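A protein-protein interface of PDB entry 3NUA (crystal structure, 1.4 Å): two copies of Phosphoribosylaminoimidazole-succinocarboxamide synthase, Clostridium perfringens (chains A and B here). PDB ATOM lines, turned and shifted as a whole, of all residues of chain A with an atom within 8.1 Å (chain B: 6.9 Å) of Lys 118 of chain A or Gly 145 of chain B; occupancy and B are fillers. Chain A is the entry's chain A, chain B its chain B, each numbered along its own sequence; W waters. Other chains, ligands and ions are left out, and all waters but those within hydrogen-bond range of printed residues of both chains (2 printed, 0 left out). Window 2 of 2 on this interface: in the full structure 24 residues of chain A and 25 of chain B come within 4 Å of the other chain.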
ATOM      1  N   ARG A  98      -3.112 -15.908 -10.194  1.00  0.00           N
ATOM      2  CA  ARG A  98      -3.590 -16.853  -9.178  1.00  0.00           C
ATOM      3  C   ARG A  98      -4.851 -17.505  -9.693  1.00  0.00           C
ATOM      4  O   ARG A  98      -5.865 -16.841  -9.886  1.00  0.00           O
ATOM      5  CB  ARG A  98      -3.833 -16.195  -7.810  1.00  0.00           C
ATOM      6  CG  ARG A  98      -2.697 -15.312  -7.319  1.00  0.00           C
ATOM      7  CD  ARG A  98      -3.049 -14.678  -5.943  1.00  0.00           C
ATOM      8  NE  ARG A  98      -1.957 -13.790  -5.557  1.00  0.00           N
ATOM      9  CZ  ARG A  98      -0.868 -14.159  -4.892  1.00  0.00           C
ATOM     10  NH1 ARG A  98      -0.738 -15.404  -4.423  1.00  0.00           N
ATOM     11  NH2 ARG A  98       0.094 -13.261  -4.683  1.00  0.00           N
ATOM     12  N   ASN A  99      -4.779 -18.808  -9.927  1.00  0.00           N
ATOM     13  CA  ASN A  99      -5.966 -19.582 -10.299  1.00  0.00           C
ATOM     14  C   ASN A  99      -6.753 -20.008  -9.084  1.00  0.00           C
ATOM     15  O   ASN A  99      -7.972 -20.172  -9.153  1.00  0.00           O
ATOM     16  CB  ASN A  99      -5.528 -20.816 -11.105  1.00  0.00           C
ATOM     17  CG  ASN A  99      -4.925 -20.440 -12.436  1.00  0.00           C
ATOM     18  OD1 ASN A  99      -3.791 -20.865 -12.809  1.00  0.00           O
ATOM     19  ND2 ASN A  99      -5.626 -19.609 -13.136  1.00  0.00           N
ATOM     20  N   MET A 105      -1.919 -13.897  -0.952  1.00  0.00           N
ATOM     21  CA  MET A 105      -3.290 -13.469  -1.121  1.00  0.00           C
ATOM     22  C   MET A 105      -4.153 -14.098  -0.051  1.00  0.00           C
ATOM     23  O   MET A 105      -4.948 -13.408   0.574  1.00  0.00           O
ATOM     24  CB  MET A 105      -3.812 -13.793  -2.522  1.00  0.00           C
ATOM     25  CG  MET A 105      -5.311 -13.428  -2.634  1.00  0.00           C
ATOM     26  SD  MET A 105      -6.072 -13.891  -4.208  1.00  0.00           S
ATOM     27  CE  MET A 105      -7.714 -13.149  -3.962  1.00  0.00           C
ATOM     28  N   TYR A 115      -8.755 -21.697  -1.469  1.00  0.00           N
ATOM     29  CA  TYR A 115     -10.005 -20.981  -1.725  1.00  0.00           C
ATOM     30  C   TYR A 115     -10.234 -20.809  -3.220  1.00  0.00           C
ATOM     31  O   TYR A 115      -9.357 -20.323  -3.956  1.00  0.00           O
ATOM     32  CB  TYR A 115      -9.970 -19.625  -1.016  1.00  0.00           C
ATOM     33  CG  TYR A 115     -11.184 -18.749  -1.207  1.00  0.00           C
ATOM     34  CD1 TYR A 115     -12.192 -18.746  -0.274  1.00  0.00           C
ATOM     35  CD2 TYR A 115     -11.272 -17.864  -2.278  1.00  0.00           C
ATOM     36  CE1 TYR A 115     -13.291 -17.933  -0.419  1.00  0.00           C
ATOM     37  CE2 TYR A 115     -12.370 -17.039  -2.440  1.00  0.00           C
ATOM     38  CZ  TYR A 115     -13.369 -17.079  -1.504  1.00  0.00           C
ATOM     39  OH  TYR A 115     -14.470 -16.264  -1.652  1.00  0.00           O
ATOM     40  N   GLU A 116     -11.427 -21.201  -3.668  1.00  0.00           N
ATOM     41  CA  GLU A 116     -11.775 -21.105  -5.080  1.00  0.00           C
ATOM     42  C   GLU A 116     -12.221 -19.709  -5.427  1.00  0.00           C
ATOM     43  O   GLU A 116     -13.097 -19.138  -4.770  1.00  0.00           O
ATOM     44  CB  GLU A 116     -12.871 -22.108  -5.418  1.00  0.00           C
ATOM     45  CG  GLU A 116     -12.387 -23.537  -5.284  1.00  0.00           C
ATOM     46  CD  GLU A 116     -13.514 -24.549  -5.371  1.00  0.00           C
ATOM     47  OE1 GLU A 116     -14.132 -24.669  -6.454  1.00  0.00           O
ATOM     48  OE2 GLU A 116     -13.786 -25.215  -4.346  1.00  0.00           O
ATOM     49  N   LEU A 117     -11.571 -19.142  -6.430  1.00  0.00           N
ATOM     50  CA  LEU A 117     -11.798 -17.762  -6.827  1.00  0.00           C
ATOM     51  C   LEU A 117     -12.875 -17.669  -7.888  1.00  0.00           C
ATOM     52  O   LEU A 117     -12.969 -18.526  -8.766  1.00  0.00           O
ATOM     53  CB  LEU A 117     -10.481 -17.175  -7.373  1.00  0.00           C
ATOM     54  CG  LEU A 117      -9.375 -16.990  -6.316  1.00  0.00           C
ATOM     55  CD1 LEU A 117      -8.001 -16.783  -6.962  1.00  0.00           C
ATOM     56  CD2 LEU A 117      -9.711 -15.784  -5.464  1.00  0.00           C
ATOM     57  N   LYS A 118     -13.659 -16.602  -7.841  1.00  0.00           N
ATOM     58  CA  LYS A 118     -14.713 -16.424  -8.829  1.00  0.00           C
ATOM     59  C   LYS A 118     -14.169 -15.969 -10.183  1.00  0.00           C
ATOM     60  O   LYS A 118     -14.889 -16.044 -11.190  1.00  0.00           O
ATOM     61  CB  LYS A 118     -15.750 -15.411  -8.329  1.00  0.00           C
ATOM     62  CG  LYS A 118     -16.590 -15.904  -7.158  1.00  0.00           C
ATOM     63  CD  LYS A 118     -17.550 -14.827  -6.656  1.00  0.00           C
ATOM     64  CE  LYS A 118     -18.821 -14.712  -7.481  1.00  0.00           C
ATOM     65  NZ  LYS A 118     -19.754 -13.656  -6.930  1.00  0.00           N
ATOM     66  N   THR A 119     -12.937 -15.453 -10.206  1.00  0.00           N
ATOM     67  CA  THR A 119     -12.297 -15.040 -11.446  1.00  0.00           C
ATOM     68  C   THR A 119     -10.804 -15.272 -11.286  1.00  0.00           C
ATOM     69  O   THR A 119     -10.290 -15.204 -10.160  1.00  0.00           O
ATOM     70  CB  THR A 119     -12.618 -13.545 -11.800  1.00  0.00           C
ATOM     71  OG1 THR A 119     -12.312 -13.294 -13.168  1.00  0.00           O
ATOM     72  CG2 THR A 119     -11.839 -12.566 -10.947  1.00  0.00           C
ATOM     73  N   THR A 120     -10.127 -15.525 -12.390  1.00  0.00           N
ATOM     74  CA  THR A 120      -8.657 -15.679 -12.349  1.00  0.00           C
ATOM     75  C   THR A 120      -8.050 -14.347 -11.918  1.00  0.00           C
ATOM     76  O   THR A 120      -8.412 -13.284 -12.432  1.00  0.00           O
ATOM     77  CB  THR A 120      -8.112 -16.022 -13.737  1.00  0.00           C
ATOM     78  OG1 THR A 120      -8.786 -17.177 -14.248  1.00  0.00           O
ATOM     79  CG2 THR A 120      -6.579 -16.285 -13.715  1.00  0.00           C
ATOM     80  N   VAL A 121      -7.154 -14.392 -10.924  1.00  0.00           N
ATOM     81  CA  VAL A 121      -6.515 -13.163 -10.458  1.00  0.00           C
ATOM     82  C   VAL A 121      -5.270 -12.860 -11.296  1.00  0.00           C
ATOM     83  O   VAL A 121      -4.437 -13.756 -11.538  1.00  0.00           O
ATOM     84  CB  VAL A 121      -6.161 -13.299  -8.984  1.00  0.00           C
ATOM     85  CG1 VAL A 121      -5.149 -12.227  -8.547  1.00  0.00           C
ATOM     86  CG2 VAL A 121      -7.439 -13.153  -8.151  1.00  0.00           C
ATOM     87  N   PRO B  92     -18.417  -3.469   0.184  1.00  0.00           N
ATOM     88  CA  PRO B  92     -17.336  -3.502   1.196  1.00  0.00           C
ATOM     89  C   PRO B  92     -15.958  -3.152   0.624  1.00  0.00           C
ATOM     90  O   PRO B  92     -14.975  -3.893   0.798  1.00  0.00           O
ATOM     91  CB  PRO B  92     -17.393  -4.930   1.716  1.00  0.00           C
ATOM     92  CG  PRO B  92     -17.866  -5.752   0.509  1.00  0.00           C
ATOM     93  CD  PRO B  92     -18.904  -4.822  -0.162  1.00  0.00           C
ATOM     94  N   TYR B 139      -9.470  -7.769  -9.646  1.00  0.00           N
ATOM     95  CA  TYR B 139      -9.601  -9.229  -9.726  1.00  0.00           C
ATOM     96  C   TYR B 139      -9.718  -9.848  -8.353  1.00  0.00           C
ATOM     97  O   TYR B 139     -10.474 -10.781  -8.163  1.00  0.00           O
ATOM     98  CB  TYR B 139      -8.457  -9.867 -10.505  1.00  0.00           C
ATOM     99  CG  TYR B 139      -8.422  -9.421 -11.937  1.00  0.00           C
ATOM    100  CD1 TYR B 139      -9.223 -10.047 -12.894  1.00  0.00           C
ATOM    101  CD2 TYR B 139      -7.625  -8.370 -12.342  1.00  0.00           C
ATOM    102  CE1 TYR B 139      -9.222  -9.642 -14.208  1.00  0.00           C
ATOM    103  CE2 TYR B 139      -7.616  -7.957 -13.658  1.00  0.00           C
ATOM    104  CZ  TYR B 139      -8.419  -8.603 -14.584  1.00  0.00           C
ATOM    105  OH  TYR B 139      -8.420  -8.197 -15.907  1.00  0.00           O
ATOM    106  N   HIS B 140      -8.975  -9.321  -7.368  1.00  0.00           N
ATOM    107  CA  HIS B 140      -9.177  -9.822  -6.011  1.00  0.00           C
ATOM    108  C   HIS B 140     -10.621  -9.562  -5.580  1.00  0.00           C
ATOM    109  O   HIS B 140     -11.264 -10.423  -4.964  1.00  0.00           O
ATOM    110  CB  HIS B 140      -8.268  -9.100  -5.025  1.00  0.00           C
ATOM    111  CG  HIS B 140      -6.806  -9.235  -5.313  1.00  0.00           C
ATOM    112  ND1 HIS B 140      -5.941  -8.169  -5.225  1.00  0.00           N
ATOM    113  CD2 HIS B 140      -6.047 -10.307  -5.650  1.00  0.00           C
ATOM    114  CE1 HIS B 140      -4.714  -8.574  -5.502  1.00  0.00           C
ATOM    115  NE2 HIS B 140      -4.746  -9.870  -5.761  1.00  0.00           N
ATOM    116  N   ALA B 141     -11.105  -8.341  -5.833  1.00  0.00           N
ATOM    117  CA  ALA B 141     -12.429  -7.928  -5.356  1.00  0.00           C
ATOM    118  C   ALA B 141     -13.512  -8.823  -5.967  1.00  0.00           C
ATOM    119  O   ALA B 141     -14.402  -9.290  -5.255  1.00  0.00           O
ATOM    120  CB  ALA B 141     -12.667  -6.478  -5.679  1.00  0.00           C
ATOM    121  N   VAL B 142     -13.438  -9.058  -7.271  1.00  0.00           N
ATOM    122  CA  VAL B 142     -14.394  -9.950  -7.928  1.00  0.00           C
ATOM    123  C   VAL B 142     -14.180 -11.385  -7.467  1.00  0.00           C
ATOM    124  O   VAL B 142     -15.110 -12.129  -7.198  1.00  0.00           O
ATOM    125  CB  VAL B 142     -14.270  -9.821  -9.459  1.00  0.00           C
ATOM    126  CG1 VAL B 142     -15.105 -10.884 -10.181  1.00  0.00           C
ATOM    127  CG2 VAL B 142     -14.735  -8.408  -9.892  1.00  0.00           C
ATOM    128  N   GLY B 143     -12.920 -11.766  -7.312  1.00  0.00           N
ATOM    129  CA  GLY B 143     -12.550 -13.132  -7.018  1.00  0.00           C
ATOM    130  C   GLY B 143     -13.065 -13.604  -5.679  1.00  0.00           C
ATOM    131  O   GLY B 143     -13.369 -14.790  -5.534  1.00  0.00           O
ATOM    132  N   ILE B 144     -13.167 -12.703  -4.695  1.00  0.00           N
ATOM    133  CA  ILE B 144     -13.669 -13.088  -3.371  1.00  0.00           C
ATOM    134  C   ILE B 144     -15.146 -12.756  -3.200  1.00  0.00           C
ATOM    135  O   ILE B 144     -15.703 -12.943  -2.106  1.00  0.00           O
ATOM    136  CB  ILE B 144     -12.853 -12.443  -2.236  1.00  0.00           C
ATOM    137  CG1 ILE B 144     -13.048 -10.928  -2.202  1.00  0.00           C
ATOM    138  CG2 ILE B 144     -11.364 -12.789  -2.425  1.00  0.00           C
ATOM    139  CD1 ILE B 144     -12.325 -10.267  -1.028  1.00  0.00           C
ATOM    140  N   GLY B 145     -15.793 -12.293  -4.276  1.00  0.00           N
ATOM    141  CA  GLY B 145     -17.236 -12.073  -4.239  1.00  0.00           C
ATOM    142  C   GLY B 145     -17.635 -10.747  -3.630  1.00  0.00           C
ATOM    143  O   GLY B 145     -18.805 -10.573  -3.287  1.00  0.00           O
ATOM    144  N   ALA B 146     -16.695  -9.806  -3.507  1.00  0.00           N
ATOM    145  CA  ALA B 146     -17.016  -8.494  -2.917  1.00  0.00           C
ATOM    146  C   ALA B 146     -17.810  -7.599  -3.884  1.00  0.00           C
ATOM    147  O   ALA B 146     -18.484  -6.665  -3.453  1.00  0.00           O
ATOM    148  CB  ALA B 146     -15.739  -7.779  -2.483  1.00  0.00           C
ATOM    149  N   THR B 147     -17.700  -7.866  -5.184  1.00  0.00           N
ATOM    150  CA  THR B 147     -18.268  -7.022  -6.223  1.00  0.00           C
ATOM    151  C   THR B 147     -18.264  -7.805  -7.534  1.00  0.00           C
ATOM    152  O   THR B 147     -17.851  -8.968  -7.576  1.00  0.00           O
ATOM    153  CB  THR B 147     -17.460  -5.692  -6.359  1.00  0.00           C
ATOM    154  OG1 THR B 147     -18.169  -4.774  -7.206  1.00  0.00           O
ATOM    155  CG2 THR B 147     -16.054  -5.943  -6.898  1.00  0.00           C
ATOM    156  N   THR B 148     -18.710  -7.155  -8.592  1.00  0.00           N
ATOM    157  CA  THR B 148     -18.665  -7.722  -9.947  1.00  0.00           C
ATOM    158  C   THR B 148     -17.909  -6.757 -10.848  1.00  0.00           C
ATOM    159  O   THR B 148     -17.734  -5.581 -10.510  1.00  0.00           O
ATOM    160  CB  THR B 148     -20.057  -7.928 -10.555  1.00  0.00           C
ATOM    161  OG1 THR B 148     -20.657  -6.640 -10.738  1.00  0.00           O
ATOM    162  CG2 THR B 148     -20.925  -8.788  -9.663  1.00  0.00           C
ATOM    163  N   PHE B 149     -17.462  -7.222 -12.005  1.00  0.00           N
ATOM    164  CA  PHE B 149     -16.782  -6.294 -12.913  1.00  0.00           C
ATOM    165  C   PHE B 149     -17.662  -5.129 -13.301  1.00  0.00           C
ATOM    166  O   PHE B 149     -17.194  -3.999 -13.394  1.00  0.00           O
ATOM    167  CB  PHE B 149     -16.247  -6.988 -14.165  1.00  0.00           C
ATOM    168  CG  PHE B 149     -15.119  -7.960 -13.892  1.00  0.00           C
ATOM    169  CD1 PHE B 149     -13.871  -7.528 -13.406  1.00  0.00           C
ATOM    170  CD2 PHE B 149     -15.300  -9.316 -14.188  1.00  0.00           C
ATOM    171  CE1 PHE B 149     -12.830  -8.465 -13.184  1.00  0.00           C
ATOM    172  CE2 PHE B 149     -14.263 -10.240 -13.983  1.00  0.00           C
ATOM    173  CZ  PHE B 149     -13.046  -9.812 -13.479  1.00  0.00           C
HETATM  174  O   HOH W   1     -15.752 -15.898  -3.874  1.00  0.00           O
HETATM  175  O   HOH W   2     -17.801 -11.706  -7.774  1.00  0.00           O
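The backbone carbonyl oxygen (O) of Gly 143 of chain B sits at hydrogen-bond distance from the backbone NH (N) of Lys 118 of chain A.
N of Arg 98 of chain A sits at hydrogen-bond distance from O of Val 121 of chain A.
Among the printed residues, pairs that only touch across the chains: Thr 120 of chain A with Tyr 139 of chain B, Lys 118 of chain A with Val 142 of chain B, Tyr 115 of chain A with Ile 144 of chain B, Thr 119 of chain A with Phe 149 of chain B, Thr 119 of chain A with Tyr 139 of chain B, Val 121 of chain A with His 140 of chain B, Leu 117 of chain A with Gly 143 of chain B, Lys 118 of chain A with Gly 145 of chain B, Met 105 of chain A with His 140 of chain B, Thr 119 of chain A with Val 142 of chain B, Val 121 of chain A with Tyr 139 of chain B, Thr 119 of chain A with Gly 143 of chain B, Tyr 115 of chain A with Gly 143 of chain B and Met 105 of chain A with Ile 144 of chain B.
Printed residues of chain B within 4 Å of Tyr 115 of chain A: Gly 143 (3.95 Å) and Ile 144 (3.6 Å). Of chain B, only Val 142, Gly 143 and Gly 145 come within 4 Å of Lys 118 of chain A. Of the printed residues of chain A, Val 142 of chain B touches Lys 118 (3.5 Å) and Thr 119 (3.8 Å). Printed residues of chain A within 4 Å of Ile 144 of chain B: Met 105 and Tyr 115. Of the printed residues of chain A, Gly 145 of chain B touches Lys 118. No residue of chain A comes within 4 Å of Ala 146 of chain B. The nearest printed residue of chain A that does not touch Tyr 139 of chain B is Met 105 of chain A (5.6 Å).
Hydrophobic or aromatic side chains of chain B that line the printed part of chain A: Tyr 139, His 140, Val 142, Ile 144 and Phe 149. Hydrophobic or aromatic side chains of chain A within 4 Å of the printed part of chain B: Met 105, Tyr 115, Leu 117 and Val 121. Among the printed residues, 15 pairs touch across the chains. Among the printed residues, no Asp or Glu carboxylate lies within 4 Å of a Lys or Arg side-chain nitrogen of the other chain.
No position is printed for both chains. Of the 15 pairs that touch across the chains among the printed residues, none has its exchanged pair printed and touching as well.
Water W1 lies within hydrogen-bond range of the side-chain hydroxyl of Tyr 115 of chain A (2.6 Å), the backbone carbonyl oxygen of Gly 143 of chain B (3.1 Å) and the backbone carbonyl oxygen of Ile 144 of chain B (3.4 Å). Water W2 lies within hydrogen-bond range of the backbone carbonyl oxygen (O) of Thr 147 of chain B (2.7 Å), the backbone carbonyl oxygen (O) of Val 142 of chain B (2.8 Å) and the side-chain amino group (NZ) of Lys 118 of chain A (2.9 Å).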
